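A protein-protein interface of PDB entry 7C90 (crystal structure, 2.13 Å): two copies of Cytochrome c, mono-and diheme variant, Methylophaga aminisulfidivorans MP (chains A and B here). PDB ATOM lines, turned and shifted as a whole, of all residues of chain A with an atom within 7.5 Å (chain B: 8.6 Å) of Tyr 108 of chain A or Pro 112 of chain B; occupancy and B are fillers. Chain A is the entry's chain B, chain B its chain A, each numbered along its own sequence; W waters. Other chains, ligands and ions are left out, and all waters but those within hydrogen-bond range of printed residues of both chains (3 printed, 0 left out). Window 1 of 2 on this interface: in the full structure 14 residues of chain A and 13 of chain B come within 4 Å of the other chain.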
ATOM      1  N   PRO A 102      32.294  11.738  -4.604  1.00  0.00           N
ATOM      2  CA  PRO A 102      32.855  11.951  -3.271  1.00  0.00           C
ATOM      3  C   PRO A 102      34.300  12.473  -3.176  1.00  0.00           C
ATOM      4  O   PRO A 102      35.130  12.215  -4.030  1.00  0.00           O
ATOM      5  CB  PRO A 102      32.783  10.566  -2.611  1.00  0.00           C
ATOM      6  CG  PRO A 102      32.578   9.593  -3.757  1.00  0.00           C
ATOM      7  CD  PRO A 102      31.802  10.362  -4.809  1.00  0.00           C
ATOM      8  N   ALA A 103      34.578  13.132  -2.047  1.00  0.00           N
ATOM      9  CA  ALA A 103      35.931  13.386  -1.526  1.00  0.00           C
ATOM     10  C   ALA A 103      36.678  12.049  -1.497  1.00  0.00           C
ATOM     11  O   ALA A 103      36.065  11.028  -1.146  1.00  0.00           O
ATOM     12  CB  ALA A 103      35.825  14.007  -0.160  1.00  0.00           C
ATOM     13  N   LEU A 104      37.934  12.047  -1.932  1.00  0.00           N
ATOM     14  CA  LEU A 104      38.769  10.828  -1.973  1.00  0.00           C
ATOM     15  C   LEU A 104      39.883  10.934  -0.918  1.00  0.00           C
ATOM     16  O   LEU A 104      40.480   9.919  -0.639  1.00  0.00           O
ATOM     17  CB  LEU A 104      39.313  10.669  -3.393  1.00  0.00           C
ATOM     18  CG  LEU A 104      38.282  10.495  -4.502  1.00  0.00           C
ATOM     19  CD1 LEU A 104      38.984  10.328  -5.834  1.00  0.00           C
ATOM     20  CD2 LEU A 104      37.354   9.322  -4.254  1.00  0.00           C
ATOM     21  N   GLY A 105      40.146  12.123  -0.352  1.00  0.00           N
ATOM     22  CA  GLY A 105      41.258  12.352   0.598  1.00  0.00           C
ATOM     23  C   GLY A 105      40.848  12.173   2.054  1.00  0.00           C
ATOM     24  O   GLY A 105      41.713  12.298   2.927  1.00  0.00           O
ATOM     25  N   ASP A 106      39.571  11.925   2.328  1.00  0.00           N
ATOM     26  CA  ASP A 106      39.026  11.843   3.711  1.00  0.00           C
ATOM     27  C   ASP A 106      39.085  10.375   4.140  1.00  0.00           C
ATOM     28  O   ASP A 106      39.440   9.549   3.286  1.00  0.00           O
ATOM     29  CB  ASP A 106      37.602  12.391   3.793  1.00  0.00           C
ATOM     30  CG  ASP A 106      36.607  11.596   2.968  1.00  0.00           C
ATOM     31  OD1 ASP A 106      37.045  10.955   1.967  1.00  0.00           O
ATOM     32  OD2 ASP A 106      35.406  11.645   3.293  1.00  0.00           O
ATOM     33  N   ASP A 107      38.740  10.044   5.385  1.00  0.00           N
ATOM     34  CA  ASP A 107      38.860   8.639   5.862  1.00  0.00           C
ATOM     35  C   ASP A 107      37.481   8.003   5.921  1.00  0.00           C
ATOM     36  O   ASP A 107      37.397   6.886   6.405  1.00  0.00           O
ATOM     37  CB  ASP A 107      39.607   8.502   7.186  1.00  0.00           C
ATOM     38  CG  ASP A 107      39.078   9.382   8.303  1.00  0.00           C
ATOM     39  OD1 ASP A 107      37.894   9.790   8.219  1.00  0.00           O
ATOM     40  OD2 ASP A 107      39.863   9.644   9.254  1.00  0.00           O
ATOM     41  N   TYR A 108      36.428   8.662   5.432  1.00  0.00           N
ATOM     42  CA  TYR A 108      35.136   7.979   5.207  1.00  0.00           C
ATOM     43  C   TYR A 108      35.118   7.501   3.753  1.00  0.00           C
ATOM     44  O   TYR A 108      35.547   8.283   2.862  1.00  0.00           O
ATOM     45  CB  TYR A 108      33.934   8.868   5.520  1.00  0.00           C
ATOM     46  CG  TYR A 108      32.659   8.141   5.204  1.00  0.00           C
ATOM     47  CD1 TYR A 108      32.159   7.160   6.050  1.00  0.00           C
ATOM     48  CD2 TYR A 108      32.013   8.339   4.002  1.00  0.00           C
ATOM     49  CE1 TYR A 108      31.039   6.414   5.717  1.00  0.00           C
ATOM     50  CE2 TYR A 108      30.892   7.608   3.655  1.00  0.00           C
ATOM     51  CZ  TYR A 108      30.390   6.650   4.519  1.00  0.00           C
ATOM     52  OH  TYR A 108      29.236   5.983   4.200  1.00  0.00           O
ATOM     53  N   TYR A 109      34.618   6.285   3.503  1.00  0.00           N
ATOM     54  CA  TYR A 109      34.508   5.709   2.136  1.00  0.00           C
ATOM     55  C   TYR A 109      33.084   5.220   1.917  1.00  0.00           C
ATOM     56  O   TYR A 109      32.554   4.615   2.789  1.00  0.00           O
ATOM     57  CB  TYR A 109      35.493   4.551   1.960  1.00  0.00           C
ATOM     58  CG  TYR A 109      36.950   4.912   2.121  1.00  0.00           C
ATOM     59  CD1 TYR A 109      37.531   5.010   3.379  1.00  0.00           C
ATOM     60  CD2 TYR A 109      37.759   5.143   1.017  1.00  0.00           C
ATOM     61  CE1 TYR A 109      38.868   5.362   3.527  1.00  0.00           C
ATOM     62  CE2 TYR A 109      39.101   5.488   1.143  1.00  0.00           C
ATOM     63  CZ  TYR A 109      39.668   5.566   2.406  1.00  0.00           C
ATOM     64  OH  TYR A 109      40.985   5.910   2.564  1.00  0.00           O
ATOM     65  N   THR A 110      32.479   5.502   0.773  1.00  0.00           N
ATOM     66  CA  THR A 110      31.173   4.936   0.415  1.00  0.00           C
ATOM     67  C   THR A 110      31.326   3.417   0.406  1.00  0.00           C
ATOM     68  O   THR A 110      30.415   2.745   0.854  1.00  0.00           O
ATOM     69  CB  THR A 110      30.660   5.474  -0.927  1.00  0.00           C
ATOM     70  OG1 THR A 110      30.534   6.891  -0.821  1.00  0.00           O
ATOM     71  CG2 THR A 110      29.338   4.849  -1.313  1.00  0.00           C
ATOM     72  N   TYR A 111      32.448   2.934  -0.124  1.00  0.00           N
ATOM     73  CA  TYR A 111      32.784   1.501  -0.238  1.00  0.00           C
ATOM     74  C   TYR A 111      34.065   1.266   0.540  1.00  0.00           C
ATOM     75  O   TYR A 111      35.149   1.579   0.057  1.00  0.00           O
ATOM     76  CB  TYR A 111      32.963   1.116  -1.704  1.00  0.00           C
ATOM     77  CG  TYR A 111      31.787   1.452  -2.565  1.00  0.00           C
ATOM     78  CD1 TYR A 111      30.609   0.738  -2.460  1.00  0.00           C
ATOM     79  CD2 TYR A 111      31.843   2.481  -3.479  1.00  0.00           C
ATOM     80  CE1 TYR A 111      29.525   1.036  -3.260  1.00  0.00           C
ATOM     81  CE2 TYR A 111      30.772   2.785  -4.289  1.00  0.00           C
ATOM     82  CZ  TYR A 111      29.606   2.046  -4.194  1.00  0.00           C
ATOM     83  OH  TYR A 111      28.549   2.312  -5.019  1.00  0.00           O
ATOM     84  N   PRO A 112      33.969   0.742   1.778  1.00  0.00           N
ATOM     85  CA  PRO A 112      35.126   0.657   2.666  1.00  0.00           C
ATOM     86  C   PRO A 112      36.340  -0.132   2.126  1.00  0.00           C
ATOM     87  O   PRO A 112      37.408   0.084   2.629  1.00  0.00           O
ATOM     88  CB  PRO A 112      34.551   0.031   3.966  1.00  0.00           C
ATOM     89  CG  PRO A 112      33.197  -0.524   3.575  1.00  0.00           C
ATOM     90  CD  PRO A 112      32.718   0.310   2.413  1.00  0.00           C
ATOM     91  N   TYR A 155      46.031  12.295   1.173  1.00  0.00           N
ATOM     92  CA  TYR A 155      45.118  11.826   2.246  1.00  0.00           C
ATOM     93  C   TYR A 155      45.283  12.689   3.500  1.00  0.00           C
ATOM     94  O   TYR A 155      46.418  12.848   3.991  1.00  0.00           O
ATOM     95  CB  TYR A 155      45.431  10.372   2.561  1.00  0.00           C
ATOM     96  CG  TYR A 155      44.669   9.755   3.693  1.00  0.00           C
ATOM     97  CD1 TYR A 155      43.341   9.400   3.565  1.00  0.00           C
ATOM     98  CD2 TYR A 155      45.319   9.468   4.877  1.00  0.00           C
ATOM     99  CE1 TYR A 155      42.663   8.785   4.603  1.00  0.00           C
ATOM    100  CE2 TYR A 155      44.663   8.847   5.923  1.00  0.00           C
ATOM    101  CZ  TYR A 155      43.331   8.508   5.786  1.00  0.00           C
ATOM    102  OH  TYR A 155      42.713   7.867   6.816  1.00  0.00           O
ATOM    103  N   GLY A 157      43.022  12.124   6.247  1.00  0.00           N
ATOM    104  CA  GLY A 157      42.331  11.380   7.309  1.00  0.00           C
ATOM    105  C   GLY A 157      43.308  10.876   8.348  1.00  0.00           C
ATOM    106  O   GLY A 157      44.490  11.301   8.304  1.00  0.00           O
ATOM    107  N   LYS A 161      43.041   4.525  10.039  1.00  0.00           N
ATOM    108  CA  LYS A 161      42.078   4.115   8.978  1.00  0.00           C
ATOM    109  C   LYS A 161      42.781   3.943   7.628  1.00  0.00           C
ATOM    110  O   LYS A 161      42.121   3.409   6.720  1.00  0.00           O
ATOM    111  CB  LYS A 161      40.938   5.132   8.913  1.00  0.00           C
ATOM    112  CG  LYS A 161      39.943   5.006  10.058  1.00  0.00           C
ATOM    113  CD  LYS A 161      38.961   6.142  10.160  1.00  0.00           C
ATOM    114  CE  LYS A 161      37.756   5.795  11.016  1.00  0.00           C
ATOM    115  NZ  LYS A 161      37.109   7.013  11.556  1.00  0.00           N
ATOM    116  N   THR B  39      25.787  19.731   5.638  1.00  0.00           N
ATOM    117  CA  THR B  39      26.411  18.417   5.374  1.00  0.00           C
ATOM    118  C   THR B  39      27.865  18.587   4.890  1.00  0.00           C
ATOM    119  O   THR B  39      28.694  17.717   5.191  1.00  0.00           O
ATOM    120  CB  THR B  39      25.514  17.683   4.371  1.00  0.00           C
ATOM    121  OG1 THR B  39      24.270  17.496   5.048  1.00  0.00           O
ATOM    122  CG2 THR B  39      26.135  16.386   3.909  1.00  0.00           C
ATOM    123  N   ASP B 107      21.995   1.074   1.049  1.00  0.00           N
ATOM    124  CA  ASP B 107      22.696   1.297   2.341  1.00  0.00           C
ATOM    125  C   ASP B 107      24.100   1.845   2.093  1.00  0.00           C
ATOM    126  O   ASP B 107      24.857   1.910   3.054  1.00  0.00           O
ATOM    127  CB  ASP B 107      22.753   0.046   3.223  1.00  0.00           C
ATOM    128  CG  ASP B 107      23.164  -1.230   2.506  1.00  0.00           C
ATOM    129  OD1 ASP B 107      23.685  -1.129   1.372  1.00  0.00           O
ATOM    130  OD2 ASP B 107      22.927  -2.311   3.078  1.00  0.00           O
ATOM    131  N   TYR B 108      24.427   2.251   0.864  1.00  0.00           N
ATOM    132  CA  TYR B 108      25.665   3.014   0.570  1.00  0.00           C
ATOM    133  C   TYR B 108      25.362   4.511   0.645  1.00  0.00           C
ATOM    134  O   TYR B 108      24.318   4.946   0.149  1.00  0.00           O
ATOM    135  CB  TYR B 108      26.216   2.606  -0.793  1.00  0.00           C
ATOM    136  CG  TYR B 108      26.568   1.144  -0.891  1.00  0.00           C
ATOM    137  CD1 TYR B 108      27.706   0.644  -0.283  1.00  0.00           C
ATOM    138  CD2 TYR B 108      25.749   0.269  -1.576  1.00  0.00           C
ATOM    139  CE1 TYR B 108      28.042  -0.691  -0.390  1.00  0.00           C
ATOM    140  CE2 TYR B 108      26.059  -1.078  -1.676  1.00  0.00           C
ATOM    141  CZ  TYR B 108      27.221  -1.551  -1.097  1.00  0.00           C
ATOM    142  OH  TYR B 108      27.541  -2.867  -1.225  1.00  0.00           O
ATOM    143  N   TYR B 109      26.240   5.266   1.278  1.00  0.00           N
ATOM    144  CA  TYR B 109      26.081   6.722   1.552  1.00  0.00           C
ATOM    145  C   TYR B 109      27.367   7.467   1.151  1.00  0.00           C
ATOM    146  O   TYR B 109      28.491   7.036   1.468  1.00  0.00           O
ATOM    147  CB  TYR B 109      25.724   6.957   3.031  1.00  0.00           C
ATOM    148  CG  TYR B 109      24.382   6.401   3.438  1.00  0.00           C
ATOM    149  CD1 TYR B 109      23.222   7.130   3.226  1.00  0.00           C
ATOM    150  CD2 TYR B 109      24.254   5.109   3.956  1.00  0.00           C
ATOM    151  CE1 TYR B 109      21.974   6.622   3.545  1.00  0.00           C
ATOM    152  CE2 TYR B 109      23.009   4.577   4.273  1.00  0.00           C
ATOM    153  CZ  TYR B 109      21.865   5.346   4.088  1.00  0.00           C
ATOM    154  OH  TYR B 109      20.615   4.853   4.369  1.00  0.00           O
ATOM    155  N   THR B 110      27.202   8.614   0.512  1.00  0.00           N
ATOM    156  CA  THR B 110      28.275   9.610   0.377  1.00  0.00           C
ATOM    157  C   THR B 110      28.589  10.199   1.760  1.00  0.00           C
ATOM    158  O   THR B 110      29.784  10.328   2.109  1.00  0.00           O
ATOM    159  CB  THR B 110      27.874  10.650  -0.666  1.00  0.00           C
ATOM    160  OG1 THR B 110      27.382   9.901  -1.777  1.00  0.00           O
ATOM    161  CG2 THR B 110      29.012  11.579  -1.008  1.00  0.00           C
ATOM    162  N   TYR B 111      27.551  10.566   2.511  1.00  0.00           N
ATOM    163  CA  TYR B 111      27.637  11.137   3.870  1.00  0.00           C
ATOM    164  C   TYR B 111      26.917  10.198   4.827  1.00  0.00           C
ATOM    165  O   TYR B 111      25.714   9.990   4.718  1.00  0.00           O
ATOM    166  CB  TYR B 111      27.084  12.559   3.847  1.00  0.00           C
ATOM    167  CG  TYR B 111      27.647  13.444   2.758  1.00  0.00           C
ATOM    168  CD1 TYR B 111      28.880  14.054   2.910  1.00  0.00           C
ATOM    169  CD2 TYR B 111      26.959  13.670   1.585  1.00  0.00           C
ATOM    170  CE1 TYR B 111      29.414  14.863   1.918  1.00  0.00           C
ATOM    171  CE2 TYR B 111      27.467  14.497   0.594  1.00  0.00           C
ATOM    172  CZ  TYR B 111      28.693  15.109   0.769  1.00  0.00           C
ATOM    173  OH  TYR B 111      29.222  15.889  -0.219  1.00  0.00           O
ATOM    174  N   PRO B 112      27.638   9.556   5.774  1.00  0.00           N
ATOM    175  CA  PRO B 112      27.028   8.569   6.676  1.00  0.00           C
ATOM    176  C   PRO B 112      25.853   9.064   7.549  1.00  0.00           C
ATOM    177  O   PRO B 112      24.918   8.279   7.847  1.00  0.00           O
ATOM    178  CB  PRO B 112      28.217   8.105   7.555  1.00  0.00           C
ATOM    179  CG  PRO B 112      29.280   9.183   7.420  1.00  0.00           C
ATOM    180  CD  PRO B 112      29.072   9.759   6.030  1.00  0.00           C
ATOM    181  N   LYS B 113      25.842  10.351   7.916  1.00  0.00           N
ATOM    182  CA  LYS B 113      24.714  10.939   8.698  1.00  0.00           C
ATOM    183  C   LYS B 113      23.395  10.762   7.940  1.00  0.00           C
ATOM    184  O   LYS B 113      22.352  10.862   8.588  1.00  0.00           O
ATOM    185  CB  LYS B 113      24.947  12.426   8.990  1.00  0.00           C
ATOM    186  CG  LYS B 113      24.888  13.331   7.769  1.00  0.00           C
ATOM    187  CD  LYS B 113      25.208  14.777   8.135  1.00  0.00           C
ATOM    188  CE  LYS B 113      24.248  15.768   7.532  1.00  0.00           C
ATOM    189  NZ  LYS B 113      24.511  17.171   7.939  1.00  0.00           N
ATOM    190  N   ASN B 114      23.417  10.547   6.617  1.00  0.00           N
ATOM    191  CA  ASN B 114      22.172  10.465   5.817  1.00  0.00           C
ATOM    192  C   ASN B 114      21.446   9.139   6.112  1.00  0.00           C
ATOM    193  O   ASN B 114      20.277   9.012   5.701  1.00  0.00           O
ATOM    194  CB  ASN B 114      22.404  10.759   4.328  1.00  0.00           C
ATOM    195  CG  ASN B 114      22.760  12.217   4.099  1.00  0.00           C
ATOM    196  OD1 ASN B 114      22.252  13.100   4.806  1.00  0.00           O
ATOM    197  ND2 ASN B 114      23.641  12.483   3.136  1.00  0.00           N
ATOM    198  N   ALA B 115      22.045   8.238   6.898  1.00  0.00           N
ATOM    199  CA  ALA B 115      21.372   7.004   7.387  1.00  0.00           C
ATOM    200  C   ALA B 115      20.362   7.340   8.495  1.00  0.00           C
ATOM    201  O   ALA B 115      19.493   6.473   8.802  1.00  0.00           O
ATOM    202  CB  ALA B 115      22.386   6.001   7.867  1.00  0.00           C
ATOM    203  N   ASN B 116      20.431   8.542   9.078  1.00  0.00           N
ATOM    204  CA  ASN B 116      19.447   8.959  10.109  1.00  0.00           C
ATOM    205  C   ASN B 116      18.664  10.171   9.583  1.00  0.00           C
ATOM    206  O   ASN B 116      19.121  10.827   8.616  1.00  0.00           O
ATOM    207  CB  ASN B 116      20.147   9.120  11.463  1.00  0.00           C
ATOM    208  CG  ASN B 116      21.051  10.328  11.547  1.00  0.00           C
ATOM    209  OD1 ASN B 116      20.606  11.474  11.417  1.00  0.00           O
ATOM    210  ND2 ASN B 116      22.332  10.073  11.764  1.00  0.00           N
ATOM    211  N   ASP B 117      17.491  10.444  10.165  1.00  0.00           N
ATOM    212  CA  ASP B 117      16.555  11.452   9.619  1.00  0.00           C
ATOM    213  C   ASP B 117      17.073  12.876   9.897  1.00  0.00           C
ATOM    214  O   ASP B 117      16.823  13.763   9.039  1.00  0.00           O
ATOM    215  CB  ASP B 117      15.122  11.186  10.083  1.00  0.00           C
ATOM    216  CG  ASP B 117      14.470  10.030   9.323  1.00  0.00           C
ATOM    217  OD1 ASP B 117      14.937   9.710   8.192  1.00  0.00           O
ATOM    218  OD2 ASP B 117      13.515   9.454   9.876  1.00  0.00           O
ATOM    219  N   GLY B 119      20.242  13.874   9.795  1.00  0.00           N
ATOM    220  CA  GLY B 119      21.238  14.122   8.739  1.00  0.00           C
ATOM    221  C   GLY B 119      20.585  14.293   7.372  1.00  0.00           C
ATOM    222  O   GLY B 119      20.957  15.219   6.650  1.00  0.00           O
ATOM    223  N   LEU B 120      19.629  13.436   7.026  1.00  0.00           N
ATOM    224  CA  LEU B 120      18.926  13.464   5.720  1.00  0.00           C
ATOM    225  C   LEU B 120      18.254  14.819   5.548  1.00  0.00           C
ATOM    226  O   LEU B 120      18.372  15.388   4.448  1.00  0.00           O
ATOM    227  CB  LEU B 120      17.893  12.339   5.656  1.00  0.00           C
ATOM    228  CG  LEU B 120      17.150  12.188   4.330  1.00  0.00           C
ATOM    229  CD1 LEU B 120      18.099  12.075   3.157  1.00  0.00           C
ATOM    230  CD2 LEU B 120      16.225  10.981   4.399  1.00  0.00           C
ATOM    231  N   THR B 123      20.830  17.464   4.748  1.00  0.00           N
ATOM    232  CA  THR B 123      21.406  17.362   3.392  1.00  0.00           C
ATOM    233  C   THR B 123      20.392  18.007   2.434  1.00  0.00           C
ATOM    234  O   THR B 123      20.783  18.784   1.554  1.00  0.00           O
ATOM    235  CB  THR B 123      21.784  15.916   3.063  1.00  0.00           C
ATOM    236  OG1 THR B 123      22.828  15.473   3.924  1.00  0.00           O
ATOM    237  CG2 THR B 123      22.197  15.746   1.616  1.00  0.00           C
ATOM    238  N   ARG B 152      12.563   6.796   2.565  1.00  0.00           N
ATOM    239  CA  ARG B 152      12.784   5.659   3.499  1.00  0.00           C
ATOM    240  C   ARG B 152      11.907   4.467   3.074  1.00  0.00           C
ATOM    241  O   ARG B 152      12.395   3.381   3.163  1.00  0.00           O
ATOM    242  CB  ARG B 152      12.516   6.058   4.946  1.00  0.00           C
ATOM    243  CG  ARG B 152      13.433   7.151   5.453  1.00  0.00           C
ATOM    244  CD  ARG B 152      14.912   6.870   5.259  1.00  0.00           C
ATOM    245  NE  ARG B 152      15.630   7.770   6.144  1.00  0.00           N
ATOM    246  CZ  ARG B 152      16.926   8.045   6.097  1.00  0.00           C
ATOM    247  NH1 ARG B 152      17.703   7.497   5.182  1.00  0.00           N
ATOM    248  NH2 ARG B 152      17.425   8.915   6.952  1.00  0.00           N
ATOM    249  N   LYS B 161      21.661  -1.323   8.842  1.00  0.00           N
ATOM    250  CA  LYS B 161      22.294  -0.012   8.531  1.00  0.00           C
ATOM    251  C   LYS B 161      21.221   1.088   8.538  1.00  0.00           C
ATOM    252  O   LYS B 161      21.622   2.236   8.377  1.00  0.00           O
ATOM    253  CB  LYS B 161      23.072  -0.068   7.211  1.00  0.00           C
ATOM    254  CG  LYS B 161      24.182  -1.112   7.158  1.00  0.00           C
ATOM    255  CD  LYS B 161      25.263  -0.835   6.120  1.00  0.00           C
ATOM    256  CE  LYS B 161      25.671  -2.057   5.316  1.00  0.00           C
ATOM    257  NZ  LYS B 161      26.366  -1.693   4.055  1.00  0.00           N
ATOM    258  N   ASP B 163      19.487   3.465  10.230  1.00  0.00           N
ATOM    259  CA  ASP B 163      19.606   4.145  11.547  1.00  0.00           C
ATOM    260  C   ASP B 163      18.284   4.818  11.932  1.00  0.00           C
ATOM    261  O   ASP B 163      18.073   4.955  13.130  1.00  0.00           O
ATOM    262  CB  ASP B 163      20.824   5.069  11.606  1.00  0.00           C
ATOM    263  CG  ASP B 163      22.147   4.313  11.592  1.00  0.00           C
ATOM    264  OD1 ASP B 163      22.175   3.153  12.061  1.00  0.00           O
ATOM    265  OD2 ASP B 163      23.149   4.883  11.105  1.00  0.00           O
HETATM  266  O   HOH W   1      29.511   7.843  -3.070  1.00  0.00           O
HETATM  267  O   HOH W   2      32.083   9.019   0.384  1.00  0.00           O
HETATM  268  O   HOH W   3      28.346   3.660   2.515  1.00  0.00           O
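The side-chain hydroxyl of Thr 110 of chain A sits at hydrogen-bond distance from the backbone carbonyl oxygen of Tyr 109 of chain B, 3.1 Å away.
O of Tyr 109 of chain B sits at hydrogen-bond distance from OH of Tyr 108 of chain A, at 3.0 Å.
Of chain B, only Tyr 109 (3.0 Å), Thr 110 (3.3 Å) and Pro 112 (3.7 Å) come within 4 Å of Tyr 108 of chain A.
Of the printed residues of chain B, Thr 110 of chain A touches Tyr 108, Tyr 109 and Thr 110.
Of the printed residues of chain A, Tyr 108 of chain B touches Thr 110 and Tyr 111.
Asp 117 of chain B touches none of the printed residues of chain A.
The nearest residue of chain B that does not touch Tyr 108 of chain A is Tyr 111 of chain B (4.6 Å).
The nearest residue of chain A that does not touch Pro 112 of chain B is Tyr 109 of chain A (7.0 Å).
Thr 110 of chain B touches Tyr 108 of chain A (O to CE2, 3.3 Å).
CE2 of Tyr 108 of chain A touches CD of Pro 112 of chain B (3.7 Å).
Thr 110 of chain A touches Tyr 108 of chain B (O to CD1, 3.6 Å).
Thr 110 of chain B touches Thr 110 of chain A.
Tyr 111 of chain A touches Tyr 108 of chain B.
Tyr 108 of chain A touches Tyr 109 of chain B, but with the chains exchanged Tyr 109 of chain A does not touch Tyr 108 of chain B (7.0 Å).
Tyr 108 of chain A touches Thr 110 of chain B, and with the chains exchanged Thr 110 of chain A touches Tyr 108 of chain B.
Thr 110 of chain A touches Tyr 109 of chain B, but with the chains exchanged Tyr 109 of chain A does not touch Thr 110 of chain B (6.1 Å).
Thr 110 of chain A touches its own counterpart, Thr 110 of chain B.
Positions printed for both chains: 107, 108, 109, 110, 111, 112 and 161.
Of the 7 pairs that touch across the chains among the printed residues, 3 have their exchanged pair printed and touching as well.
Water W1 bridges the side-chain hydroxyl (OG1) of Thr 110 of chain A and the side-chain hydroxyl (OG1) of Thr 110 of chain B.
Water W3 lies within hydrogen-bond range of O of Thr 110 of chain A (2.8 Å), N of Tyr 109 of chain B (2.9 Å) and OH of Tyr 108 of chain A (3.0 Å).
Water W2 bridges OG1 of Thr 110 of chain A and O of Thr 110 of chain B.
Hydrophobic or aromatic side chains of chain A within 4 Å of the printed part of chain B: Tyr 108 and Tyr 111.
Of the 18 printed residues of chain B, 4 touch a printed residue of chain A.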
